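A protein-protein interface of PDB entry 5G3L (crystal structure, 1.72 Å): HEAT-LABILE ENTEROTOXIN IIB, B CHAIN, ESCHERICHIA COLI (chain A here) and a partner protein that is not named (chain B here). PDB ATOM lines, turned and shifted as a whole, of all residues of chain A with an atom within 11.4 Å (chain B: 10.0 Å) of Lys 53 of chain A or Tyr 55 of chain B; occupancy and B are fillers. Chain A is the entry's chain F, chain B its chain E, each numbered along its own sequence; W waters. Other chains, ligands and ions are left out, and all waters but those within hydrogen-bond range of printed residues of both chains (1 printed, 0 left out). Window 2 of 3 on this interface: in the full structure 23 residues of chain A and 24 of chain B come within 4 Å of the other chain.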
ATOM      1  N   ASP A  29      -7.888 -18.749 -18.244  1.00  0.00           N
ATOM      2  CA  ASP A  29      -7.192 -19.534 -19.295  1.00  0.00           C
ATOM      3  C   ASP A  29      -5.998 -18.732 -19.861  1.00  0.00           C
ATOM      4  O   ASP A  29      -6.185 -17.551 -20.211  1.00  0.00           O
ATOM      5  CB  ASP A  29      -8.257 -19.839 -20.374  1.00  0.00           C
ATOM      6  CG  ASP A  29      -7.765 -20.724 -21.508  1.00  0.00           C
ATOM      7  OD1 ASP A  29      -6.583 -20.676 -21.860  1.00  0.00           O
ATOM      8  OD2 ASP A  29      -8.634 -21.395 -22.130  1.00  0.00           O
ATOM      9  N   ILE A  30      -4.782 -19.325 -19.907  1.00  0.00           N
ATOM     10  CA  ILE A  30      -3.644 -18.606 -20.506  1.00  0.00           C
ATOM     11  C   ILE A  30      -3.198 -19.216 -21.847  1.00  0.00           C
ATOM     12  O   ILE A  30      -2.125 -18.897 -22.327  1.00  0.00           O
ATOM     13  CB  ILE A  30      -2.441 -18.396 -19.583  1.00  0.00           C
ATOM     14  CG1 ILE A  30      -1.890 -19.720 -19.048  1.00  0.00           C
ATOM     15  CG2 ILE A  30      -2.854 -17.425 -18.473  1.00  0.00           C
ATOM     16  CD1 ILE A  30      -0.504 -19.524 -18.439  1.00  0.00           C
ATOM     17  N   ASP A  35      -6.966 -17.437 -24.507  1.00  0.00           N
ATOM     18  CA  ASP A  35      -6.545 -16.784 -23.270  1.00  0.00           C
ATOM     19  C   ASP A  35      -7.580 -15.733 -22.892  1.00  0.00           C
ATOM     20  O   ASP A  35      -8.077 -14.982 -23.733  1.00  0.00           O
ATOM     21  CB  ASP A  35      -5.152 -16.187 -23.360  1.00  0.00           C
ATOM     22  CG  ASP A  35      -5.072 -15.010 -24.264  1.00  0.00           C
ATOM     23  OD1 ASP A  35      -5.318 -15.194 -25.486  1.00  0.00           O
ATOM     24  OD2 ASP A  35      -4.709 -13.909 -23.773  1.00  0.00           O
ATOM     25  N   GLY A  36      -7.928 -15.722 -21.596  1.00  0.00           N
ATOM     26  CA  GLY A  36      -8.894 -14.755 -21.109  1.00  0.00           C
ATOM     27  C   GLY A  36      -9.634 -15.241 -19.904  1.00  0.00           C
ATOM     28  O   GLY A  36      -9.334 -16.350 -19.377  1.00  0.00           O
ATOM     29  N   MET A  37     -10.607 -14.417 -19.484  1.00  0.00           N
ATOM     30  CA  MET A  37     -11.491 -14.726 -18.355  1.00  0.00           C
ATOM     31  C   MET A  37     -12.924 -14.866 -18.853  1.00  0.00           C
ATOM     32  O   MET A  37     -13.404 -14.034 -19.662  1.00  0.00           O
ATOM     33  CB  MET A  37     -11.444 -13.594 -17.296  1.00  0.00           C
ATOM     34  CG  MET A  37     -10.016 -13.312 -16.738  1.00  0.00           C
ATOM     35  SD  MET A  37      -9.417 -14.702 -15.848  1.00  0.00           S
ATOM     36  CE  MET A  37     -10.756 -15.135 -14.772  1.00  0.00           C
ATOM     37  N   ARG A  48     -17.441 -13.511 -22.182  1.00  0.00           N
ATOM     38  CA  ARG A  48     -16.038 -13.123 -21.935  1.00  0.00           C
ATOM     39  C   ARG A  48     -16.013 -11.793 -21.185  1.00  0.00           C
ATOM     40  O   ARG A  48     -16.771 -10.903 -21.529  1.00  0.00           O
ATOM     41  CB  ARG A  48     -15.265 -12.939 -23.255  1.00  0.00           C
ATOM     42  CG  ARG A  48     -13.809 -12.597 -23.070  1.00  0.00           C
ATOM     43  CD  ARG A  48     -13.285 -11.500 -23.992  1.00  0.00           C
ATOM     44  NE  ARG A  48     -13.801 -11.372 -25.334  1.00  0.00           N
ATOM     45  CZ  ARG A  48     -13.612 -10.257 -26.034  1.00  0.00           C
ATOM     46  NH1 ARG A  48     -12.908  -9.232 -25.514  1.00  0.00           N
ATOM     47  NH2 ARG A  48     -14.117 -10.144 -27.255  1.00  0.00           N
ATOM     48  N   ILE A  49     -15.139 -11.727 -20.201  1.00  0.00           N
ATOM     49  CA  ILE A  49     -14.895 -10.474 -19.453  1.00  0.00           C
ATOM     50  C   ILE A  49     -13.731  -9.767 -20.151  1.00  0.00           C
ATOM     51  O   ILE A  49     -12.737 -10.382 -20.356  1.00  0.00           O
ATOM     52  CB  ILE A  49     -14.515 -10.766 -17.979  1.00  0.00           C
ATOM     53  CG1 ILE A  49     -15.550 -11.675 -17.328  1.00  0.00           C
ATOM     54  CG2 ILE A  49     -14.321  -9.478 -17.240  1.00  0.00           C
ATOM     55  CD1 ILE A  49     -15.210 -12.164 -15.908  1.00  0.00           C
ATOM     56  N   SER A  50     -13.876  -8.494 -20.499  1.00  0.00           N
ATOM     57  CA  SER A  50     -12.741  -7.782 -21.176  1.00  0.00           C
ATOM     58  C   SER A  50     -11.616  -7.554 -20.191  1.00  0.00           C
ATOM     59  O   SER A  50     -11.810  -7.669 -18.941  1.00  0.00           O
ATOM     60  CB  SER A  50     -13.072  -6.412 -21.878  1.00  0.00           C
ATOM     61  OG  SER A  50     -14.000  -5.704 -21.085  1.00  0.00           O
ATOM     62  N   ARG A  51     -10.472  -7.242 -20.817  1.00  0.00           N
ATOM     63  CA  ARG A  51      -9.205  -6.961 -20.149  1.00  0.00           C
ATOM     64  C   ARG A  51      -8.662  -5.583 -20.585  1.00  0.00           C
ATOM     65  O   ARG A  51      -8.892  -5.161 -21.699  1.00  0.00           O
ATOM     66  CB  ARG A  51      -8.174  -7.943 -20.582  1.00  0.00           C
ATOM     67  CG  ARG A  51      -8.098  -9.252 -19.856  1.00  0.00           C
ATOM     68  CD  ARG A  51      -7.088 -10.238 -20.508  1.00  0.00           C
ATOM     69  NE  ARG A  51      -7.104 -10.274 -21.986  1.00  0.00           N
ATOM     70  CZ  ARG A  51      -6.612 -11.286 -22.702  1.00  0.00           C
ATOM     71  NH1 ARG A  51      -6.102 -12.323 -22.089  1.00  0.00           N
ATOM     72  NH2 ARG A  51      -6.662 -11.277 -24.031  1.00  0.00           N
ATOM     73  N   ALA A  52      -8.006  -4.895 -19.683  1.00  0.00           N
ATOM     74  CA  ALA A  52      -7.382  -3.588 -19.992  1.00  0.00           C
ATOM     75  C   ALA A  52      -6.194  -3.401 -19.075  1.00  0.00           C
ATOM     76  O   ALA A  52      -6.298  -3.577 -17.884  1.00  0.00           O
ATOM     77  CB  ALA A  52      -8.371  -2.474 -19.796  1.00  0.00           C
ATOM     78  N   LYS A  53      -5.060  -3.025 -19.653  1.00  0.00           N
ATOM     79  CA  LYS A  53      -3.839  -2.810 -18.883  1.00  0.00           C
ATOM     80  C   LYS A  53      -3.857  -1.482 -18.092  1.00  0.00           C
ATOM     81  O   LYS A  53      -3.346  -1.426 -16.984  1.00  0.00           O
ATOM     82  CB  LYS A  53      -2.608  -2.849 -19.789  1.00  0.00           C
ATOM     83  CG  LYS A  53      -1.301  -2.765 -19.028  1.00  0.00           C
ATOM     84  CD  LYS A  53      -0.068  -3.142 -19.894  1.00  0.00           C
ATOM     85  CE  LYS A  53       0.171  -2.095 -20.970  1.00  0.00           C
ATOM     86  NZ  LYS A  53       0.614  -0.802 -20.385  1.00  0.00           N
ATOM     87  N   ASP A  54      -4.404  -0.449 -18.680  1.00  0.00           N
ATOM     88  CA  ASP A  54      -4.274   0.917 -18.134  1.00  0.00           C
ATOM     89  C   ASP A  54      -5.539   1.501 -17.548  1.00  0.00           C
ATOM     90  O   ASP A  54      -6.636   1.031 -17.800  1.00  0.00           O
ATOM     91  CB  ASP A  54      -3.779   1.860 -19.224  1.00  0.00           C
ATOM     92  CG  ASP A  54      -2.446   1.414 -19.777  1.00  0.00           C
ATOM     93  OD1 ASP A  54      -1.606   0.914 -19.006  1.00  0.00           O
ATOM     94  OD2 ASP A  54      -2.261   1.524 -20.980  1.00  0.00           O
ATOM     95  N   TYR A  55      -5.338   2.573 -16.790  1.00  0.00           N
ATOM     96  CA  TYR A  55      -6.384   3.323 -16.181  1.00  0.00           C
ATOM     97  C   TYR A  55      -7.155   4.092 -17.241  1.00  0.00           C
ATOM     98  O   TYR A  55      -6.523   4.621 -18.178  1.00  0.00           O
ATOM     99  CB  TYR A  55      -5.759   4.240 -15.112  1.00  0.00           C
ATOM    100  CG  TYR A  55      -6.709   5.128 -14.391  1.00  0.00           C
ATOM    101  CD1 TYR A  55      -7.105   6.347 -14.935  1.00  0.00           C
ATOM    102  CD2 TYR A  55      -7.269   4.746 -13.192  1.00  0.00           C
ATOM    103  CE1 TYR A  55      -7.994   7.161 -14.288  1.00  0.00           C
ATOM    104  CE2 TYR A  55      -8.193   5.550 -12.553  1.00  0.00           C
ATOM    105  CZ  TYR A  55      -8.545   6.752 -13.075  1.00  0.00           C
ATOM    106  OH  TYR A  55      -9.452   7.551 -12.407  1.00  0.00           O
ATOM    107  N   PRO A  56      -8.483   4.184 -17.160  1.00  0.00           N
ATOM    108  CA  PRO A  56      -9.305   3.701 -16.023  1.00  0.00           C
ATOM    109  C   PRO A  56      -9.906   2.309 -16.155  1.00  0.00           C
ATOM    110  O   PRO A  56     -10.509   1.815 -15.221  1.00  0.00           O
ATOM    111  CB  PRO A  56     -10.419   4.724 -15.998  1.00  0.00           C
ATOM    112  CG  PRO A  56     -10.618   5.075 -17.426  1.00  0.00           C
ATOM    113  CD  PRO A  56      -9.249   5.132 -17.989  1.00  0.00           C
ATOM    114  N   ASP A  57      -9.793   1.707 -17.334  1.00  0.00           N
ATOM    115  CA  ASP A  57     -10.526   0.459 -17.594  1.00  0.00           C
ATOM    116  C   ASP A  57      -9.915  -0.688 -16.842  1.00  0.00           C
ATOM    117  O   ASP A  57     -10.596  -1.694 -16.636  1.00  0.00           O
ATOM    118  CB  ASP A  57     -10.621   0.135 -19.070  1.00  0.00           C
ATOM    119  CG  ASP A  57     -11.687   0.969 -19.794  1.00  0.00           C
ATOM    120  OD1 ASP A  57     -12.452   1.684 -19.166  1.00  0.00           O
ATOM    121  OD2 ASP A  57     -11.757   0.891 -21.032  1.00  0.00           O
ATOM    122  N   ASN A  58      -8.671  -0.549 -16.394  1.00  0.00           N
ATOM    123  CA  ASN A  58      -8.122  -1.590 -15.551  1.00  0.00           C
ATOM    124  C   ASN A  58      -8.890  -1.704 -14.235  1.00  0.00           C
ATOM    125  O   ASN A  58      -9.001  -2.824 -13.680  1.00  0.00           O
ATOM    126  CB  ASN A  58      -6.612  -1.415 -15.308  1.00  0.00           C
ATOM    127  CG  ASN A  58      -6.240  -0.138 -14.595  1.00  0.00           C
ATOM    128  OD1 ASN A  58      -7.042   0.705 -14.287  1.00  0.00           O
ATOM    129  ND2 ASN A  58      -4.934  -0.005 -14.338  1.00  0.00           N
ATOM    130  N   VAL A  59      -9.472  -0.624 -13.774  1.00  0.00           N
ATOM    131  CA  VAL A  59     -10.313  -0.679 -12.566  1.00  0.00           C
ATOM    132  C   VAL A  59     -11.639  -1.430 -12.826  1.00  0.00           C
ATOM    133  O   VAL A  59     -12.008  -2.392 -12.138  1.00  0.00           O
ATOM    134  CB  VAL A  59     -10.626   0.718 -12.041  1.00  0.00           C
ATOM    135  CG1 VAL A  59     -11.701   0.677 -10.940  1.00  0.00           C
ATOM    136  CG2 VAL A  59      -9.345   1.384 -11.546  1.00  0.00           C
ATOM    137  N   MET A  60     -12.367  -0.968 -13.851  1.00  0.00           N
ATOM    138  CA  MET A  60     -13.677  -1.558 -14.132  1.00  0.00           C
ATOM    139  C   MET A  60     -13.568  -3.020 -14.479  1.00  0.00           C
ATOM    140  O   MET A  60     -14.390  -3.835 -14.019  1.00  0.00           O
ATOM    141  CB  MET A  60     -14.395  -0.817 -15.269  1.00  0.00           C
ATOM    142  CG  MET A  60     -15.215   0.365 -14.797  1.00  0.00           C
ATOM    143  SD  MET A  60     -14.199   1.812 -14.359  1.00  0.00           S
ATOM    144  CE  MET A  60     -13.845   2.380 -15.962  1.00  0.00           C
ATOM    145  N   THR A  61     -12.572  -3.395 -15.257  1.00  0.00           N
ATOM    146  CA  THR A  61     -12.379  -4.829 -15.636  1.00  0.00           C
ATOM    147  C   THR A  61     -12.042  -5.674 -14.411  1.00  0.00           C
ATOM    148  O   THR A  61     -12.596  -6.771 -14.242  1.00  0.00           O
ATOM    149  CB  THR A  61     -11.360  -5.083 -16.778  1.00  0.00           C
ATOM    150  OG1 THR A  61     -10.066  -4.535 -16.429  1.00  0.00           O
ATOM    151  CG2 THR A  61     -11.903  -4.463 -18.087  1.00  0.00           C
ATOM    152  N   ALA A  62     -11.192  -5.169 -13.540  1.00  0.00           N
ATOM    153  CA  ALA A  62     -10.935  -5.878 -12.227  1.00  0.00           C
ATOM    154  C   ALA A  62     -12.226  -6.086 -11.443  1.00  0.00           C
ATOM    155  O   ALA A  62     -12.456  -7.139 -10.875  1.00  0.00           O
ATOM    156  CB  ALA A  62      -9.948  -5.121 -11.370  1.00  0.00           C
ATOM    157  N   ARG A  65     -14.414  -8.885 -12.800  1.00  0.00           N
ATOM    158  CA  ARG A  65     -13.888 -10.207 -12.335  1.00  0.00           C
ATOM    159  C   ARG A  65     -14.283 -10.492 -10.902  1.00  0.00           C
ATOM    160  O   ARG A  65     -14.643 -11.599 -10.555  1.00  0.00           O
ATOM    161  CB  ARG A  65     -12.361 -10.257 -12.491  1.00  0.00           C
ATOM    162  CG  ARG A  65     -11.912 -10.192 -13.920  1.00  0.00           C
ATOM    163  CD  ARG A  65     -10.392 -10.503 -14.047  1.00  0.00           C
ATOM    164  NE  ARG A  65      -9.541  -9.600 -13.325  1.00  0.00           N
ATOM    165  CZ  ARG A  65      -9.026  -8.482 -13.851  1.00  0.00           C
ATOM    166  NH1 ARG A  65      -9.348  -8.124 -15.084  1.00  0.00           N
ATOM    167  NH2 ARG A  65      -8.246  -7.731 -13.143  1.00  0.00           N
ATOM    168  N   ARG B  51       2.711 -19.087 -13.526  1.00  0.00           N
ATOM    169  CA  ARG B  51       3.097 -17.712 -13.251  1.00  0.00           C
ATOM    170  C   ARG B  51       3.433 -16.996 -14.543  1.00  0.00           C
ATOM    171  O   ARG B  51       3.756 -17.597 -15.571  1.00  0.00           O
ATOM    172  CB  ARG B  51       4.292 -17.614 -12.274  1.00  0.00           C
ATOM    173  CG  ARG B  51       5.556 -18.255 -12.848  1.00  0.00           C
ATOM    174  CD  ARG B  51       6.867 -17.808 -12.222  1.00  0.00           C
ATOM    175  NE  ARG B  51       7.229 -18.595 -11.083  1.00  0.00           N
ATOM    176  CZ  ARG B  51       8.465 -18.751 -10.629  1.00  0.00           C
ATOM    177  NH1 ARG B  51       9.532 -18.227 -11.259  1.00  0.00           N
ATOM    178  NH2 ARG B  51       8.624 -19.463  -9.552  1.00  0.00           N
ATOM    179  N   ALA B  52       3.328 -15.710 -14.482  1.00  0.00           N
ATOM    180  CA  ALA B  52       3.670 -14.831 -15.634  1.00  0.00           C
ATOM    181  C   ALA B  52       4.068 -13.473 -15.138  1.00  0.00           C
ATOM    182  O   ALA B  52       3.430 -12.915 -14.300  1.00  0.00           O
ATOM    183  CB  ALA B  52       2.498 -14.691 -16.582  1.00  0.00           C
ATOM    184  N   LYS B  53       5.112 -12.923 -15.718  1.00  0.00           N
ATOM    185  CA  LYS B  53       5.609 -11.623 -15.263  1.00  0.00           C
ATOM    186  C   LYS B  53       4.816 -10.415 -15.772  1.00  0.00           C
ATOM    187  O   LYS B  53       4.585  -9.451 -15.042  1.00  0.00           O
ATOM    188  CB  LYS B  53       7.076 -11.509 -15.667  1.00  0.00           C
ATOM    189  CG  LYS B  53       7.862 -10.494 -14.833  1.00  0.00           C
ATOM    190  CD  LYS B  53       9.047  -9.920 -15.615  1.00  0.00           C
ATOM    191  CE  LYS B  53      10.217  -9.448 -14.733  1.00  0.00           C
ATOM    192  NZ  LYS B  53      11.378 -10.381 -14.707  1.00  0.00           N
ATOM    193  N   ASP B  54       4.341 -10.497 -17.006  1.00  0.00           N
ATOM    194  CA  ASP B  54       3.727  -9.344 -17.679  1.00  0.00           C
ATOM    195  C   ASP B  54       2.252  -9.482 -18.009  1.00  0.00           C
ATOM    196  O   ASP B  54       1.723 -10.570 -17.995  1.00  0.00           O
ATOM    197  CB  ASP B  54       4.451  -9.087 -19.014  1.00  0.00           C
ATOM    198  CG  ASP B  54       5.919  -8.757 -18.823  1.00  0.00           C
ATOM    199  OD1 ASP B  54       6.260  -8.085 -17.825  1.00  0.00           O
ATOM    200  OD2 ASP B  54       6.718  -9.242 -19.630  1.00  0.00           O
ATOM    201  N   TYR B  55       1.651  -8.343 -18.326  1.00  0.00           N
ATOM    202  CA  TYR B  55       0.324  -8.223 -18.898  1.00  0.00           C
ATOM    203  C   TYR B  55       0.300  -8.829 -20.311  1.00  0.00           C
ATOM    204  O   TYR B  55       1.275  -8.645 -21.059  1.00  0.00           O
ATOM    205  CB  TYR B  55      -0.129  -6.749 -18.911  1.00  0.00           C
ATOM    206  CG  TYR B  55      -1.469  -6.538 -19.542  1.00  0.00           C
ATOM    207  CD1 TYR B  55      -1.615  -6.425 -20.925  1.00  0.00           C
ATOM    208  CD2 TYR B  55      -2.642  -6.503 -18.763  1.00  0.00           C
ATOM    209  CE1 TYR B  55      -2.848  -6.304 -21.498  1.00  0.00           C
ATOM    210  CE2 TYR B  55      -3.903  -6.357 -19.335  1.00  0.00           C
ATOM    211  CZ  TYR B  55      -4.013  -6.241 -20.722  1.00  0.00           C
ATOM    212  OH  TYR B  55      -5.247  -6.125 -21.267  1.00  0.00           O
ATOM    213  N   PRO B  56      -0.735  -9.583 -20.707  1.00  0.00           N
ATOM    214  CA  PRO B  56      -1.930  -9.868 -19.923  1.00  0.00           C
ATOM    215  C   PRO B  56      -1.930 -11.122 -19.040  1.00  0.00           C
ATOM    216  O   PRO B  56      -2.907 -11.328 -18.290  1.00  0.00           O
ATOM    217  CB  PRO B  56      -2.972 -10.081 -21.005  1.00  0.00           C
ATOM    218  CG  PRO B  56      -2.203 -10.737 -22.105  1.00  0.00           C
ATOM    219  CD  PRO B  56      -0.869 -10.082 -22.093  1.00  0.00           C
ATOM    220  N   ASP B  57      -0.932 -11.979 -19.195  1.00  0.00           N
ATOM    221  CA  ASP B  57      -0.950 -13.321 -18.537  1.00  0.00           C
ATOM    222  C   ASP B  57      -0.922 -13.191 -17.030  1.00  0.00           C
ATOM    223  O   ASP B  57      -1.417 -14.049 -16.329  1.00  0.00           O
ATOM    224  CB  ASP B  57       0.115 -14.265 -19.030  1.00  0.00           C
ATOM    225  CG  ASP B  57      -0.149 -14.761 -20.451  1.00  0.00           C
ATOM    226  OD1 ASP B  57      -1.287 -14.561 -20.957  1.00  0.00           O
ATOM    227  OD2 ASP B  57       0.741 -15.465 -20.967  1.00  0.00           O
ATOM    228  N   ASN B  58      -0.365 -12.095 -16.540  1.00  0.00           N
ATOM    229  CA  ASN B  58      -0.321 -11.925 -15.070  1.00  0.00           C
ATOM    230  C   ASN B  58      -1.709 -11.649 -14.456  1.00  0.00           C
ATOM    231  O   ASN B  58      -1.953 -11.864 -13.245  1.00  0.00           O
ATOM    232  CB  ASN B  58       0.749 -10.919 -14.694  1.00  0.00           C
ATOM    233  CG  ASN B  58       0.488  -9.526 -15.231  1.00  0.00           C
ATOM    234  OD1 ASN B  58      -0.605  -9.147 -15.776  1.00  0.00           O
ATOM    235  ND2 ASN B  58       1.495  -8.691 -14.998  1.00  0.00           N
ATOM    236  N   VAL B  59      -2.648 -11.177 -15.288  1.00  0.00           N
ATOM    237  CA  VAL B  59      -4.056 -11.100 -14.876  1.00  0.00           C
ATOM    238  C   VAL B  59      -4.701 -12.469 -14.671  1.00  0.00           C
ATOM    239  O   VAL B  59      -5.250 -12.823 -13.604  1.00  0.00           O
ATOM    240  CB  VAL B  59      -4.913 -10.237 -15.859  1.00  0.00           C
ATOM    241  CG1 VAL B  59      -6.384 -10.331 -15.532  1.00  0.00           C
ATOM    242  CG2 VAL B  59      -4.422  -8.785 -15.828  1.00  0.00           C
ATOM    243  N   MET B  60      -4.591 -13.276 -15.696  1.00  0.00           N
ATOM    244  CA  MET B  60      -5.120 -14.652 -15.660  1.00  0.00           C
ATOM    245  C   MET B  60      -4.475 -15.489 -14.522  1.00  0.00           C
ATOM    246  O   MET B  60      -5.173 -16.223 -13.843  1.00  0.00           O
ATOM    247  CB  MET B  60      -4.972 -15.357 -16.979  1.00  0.00           C
ATOM    248  CG  MET B  60      -6.128 -15.096 -17.962  1.00  0.00           C
ATOM    249  SD  MET B  60      -6.051 -13.465 -18.681  1.00  0.00           S
ATOM    250  CE  MET B  60      -4.806 -13.710 -19.912  1.00  0.00           C
ATOM    251  N   THR B  61      -3.175 -15.339 -14.326  1.00  0.00           N
ATOM    252  CA  THR B  61      -2.486 -16.095 -13.244  1.00  0.00           C
ATOM    253  C   THR B  61      -2.966 -15.649 -11.868  1.00  0.00           C
ATOM    254  O   THR B  61      -3.209 -16.488 -10.979  1.00  0.00           O
ATOM    255  CB  THR B  61      -0.957 -16.113 -13.378  1.00  0.00           C
ATOM    256  OG1 THR B  61      -0.447 -14.790 -13.356  1.00  0.00           O
ATOM    257  CG2 THR B  61      -0.529 -16.840 -14.674  1.00  0.00           C
HETATM  258  O   HOH W   1       0.299 -17.611 -22.351  1.00  0.00           O
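Printed residues of chain B within 4 Å of Ile 30 of chain A: Met 60 (3.3 Å).
Of the printed residues of chain B, Gly 36 of chain A touches Met 60 (3.7 Å).
Printed residues of chain B within 4 Å of Met 37 of chain A: Met 60.
Of the printed residues of chain B, Ala 52 of chain A touches Tyr 55 (3.4 Å).
Of chain B, only Tyr 55 comes within 4 Å of Lys 53 of chain A.
No residue of chain B comes within 4 Å of Asp 54 of chain A.
Ala 52 of chain B touches none of the printed residues of chain A.
Tyr 55 of chain B touches just these residues of chain A: Arg 51, Ala 52 and Lys 53.
No residue of chain A comes within 4 Å of Asp 57 of chain B.
Printed residues of chain A within 4 Å of Val 59 of chain B: Arg 65 (3.6 Å).
Of the printed residues of chain A, Met 60 of chain B touches Asp 29, Ile 30, Asp 35, Gly 36, Met 37 and Arg 51.
The nearest residue of chain B that does not touch Lys 53 of chain A is Pro 56 of chain B (6.5 Å).
The nearest residue of chain A that does not touch Tyr 55 of chain B is Asp 54 of chain A (6.0 Å).
N of Gly 36 of chain A sits at hydrogen-bond distance from O of Asp 29 of chain A, 2.9 Å away.
O of Lys 53 of chain A sits at hydrogen-bond distance from ND2 of Asn 58 of chain A (3.4 Å).
N of Ile 49 of chain A is in hydrogen-bond range of O of Met 37 of chain A, 2.9 Å away.
The side-chain amide nitrogen (ND2) of Asn 58 of chain B sits close to the backbone NH (N) of Tyr 55 of chain B, at 3.3 Å.
The side-chain amino group (NZ) of Lys 53 of chain A is in salt-bridge range of the side-chain carboxylate (OD1) of Asp 54 of chain A, at 3.1 Å.
The side-chain carboxylate (OD2) of Asp 35 of chain A lies within salt-bridge range of the guanidinium group (NH1) of Arg 51 of chain A (2.7 Å).
The side-chain hydroxyl of Tyr 55 of chain B lies within hydrogen-bond range of the backbone NH of Lys 53 of chain A (3.5 Å).
SD of Met 60 of chain B lies close to NH1 of Arg 51 of chain A (3.6 Å).
The backbone NH (N) of Ala 52 of chain A sits at hydrogen-bond distance from the side-chain hydroxyl (OH) of Tyr 55 of chain B, at 3.4 Å.
Asp 29 of chain A touches Met 60 of chain B (O to CG, 3.3 Å).
CG2 of Ile 30 of chain A touches CB of Met 60 of chain B (3.3 Å).
Asp 35 of chain A touches Met 60 of chain B.
Met 60 of chain B touches Gly 36 of chain A (CG to O, 3.7 Å).
Met 60 of chain B touches Met 37 of chain A.
Arg 51 of chain A touches Tyr 55 of chain B (CB to OH, 3.5 Å).
CB of Pro 56 of chain B touches NH1 of Arg 51 of chain A, 3.9998 Å away.
CZ of Arg 65 of chain A touches CG1 of Val 59 of chain B, 3.6 Å away.
Water W1 lies within hydrogen-bond range of the side-chain carboxylate of Asp 57 of chain B (2.6 Å) and the backbone carbonyl oxygen of Ile 30 of chain A (2.7 Å).
Printed residues of chain B that touch a printed residue of chain A: Tyr 55, Pro 56, Val 59 and Met 60.
Of the 21 printed residues of chain A, 9 touch a printed residue of chain B.
Hydrophobic or aromatic side chains of chain A that line the printed part of chain B: Ile 30 and Met 37.
Among the printed residues, no Asp or Glu carboxylate lies within 4 Å of a Lys or Arg side-chain nitrogen of the other chain.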
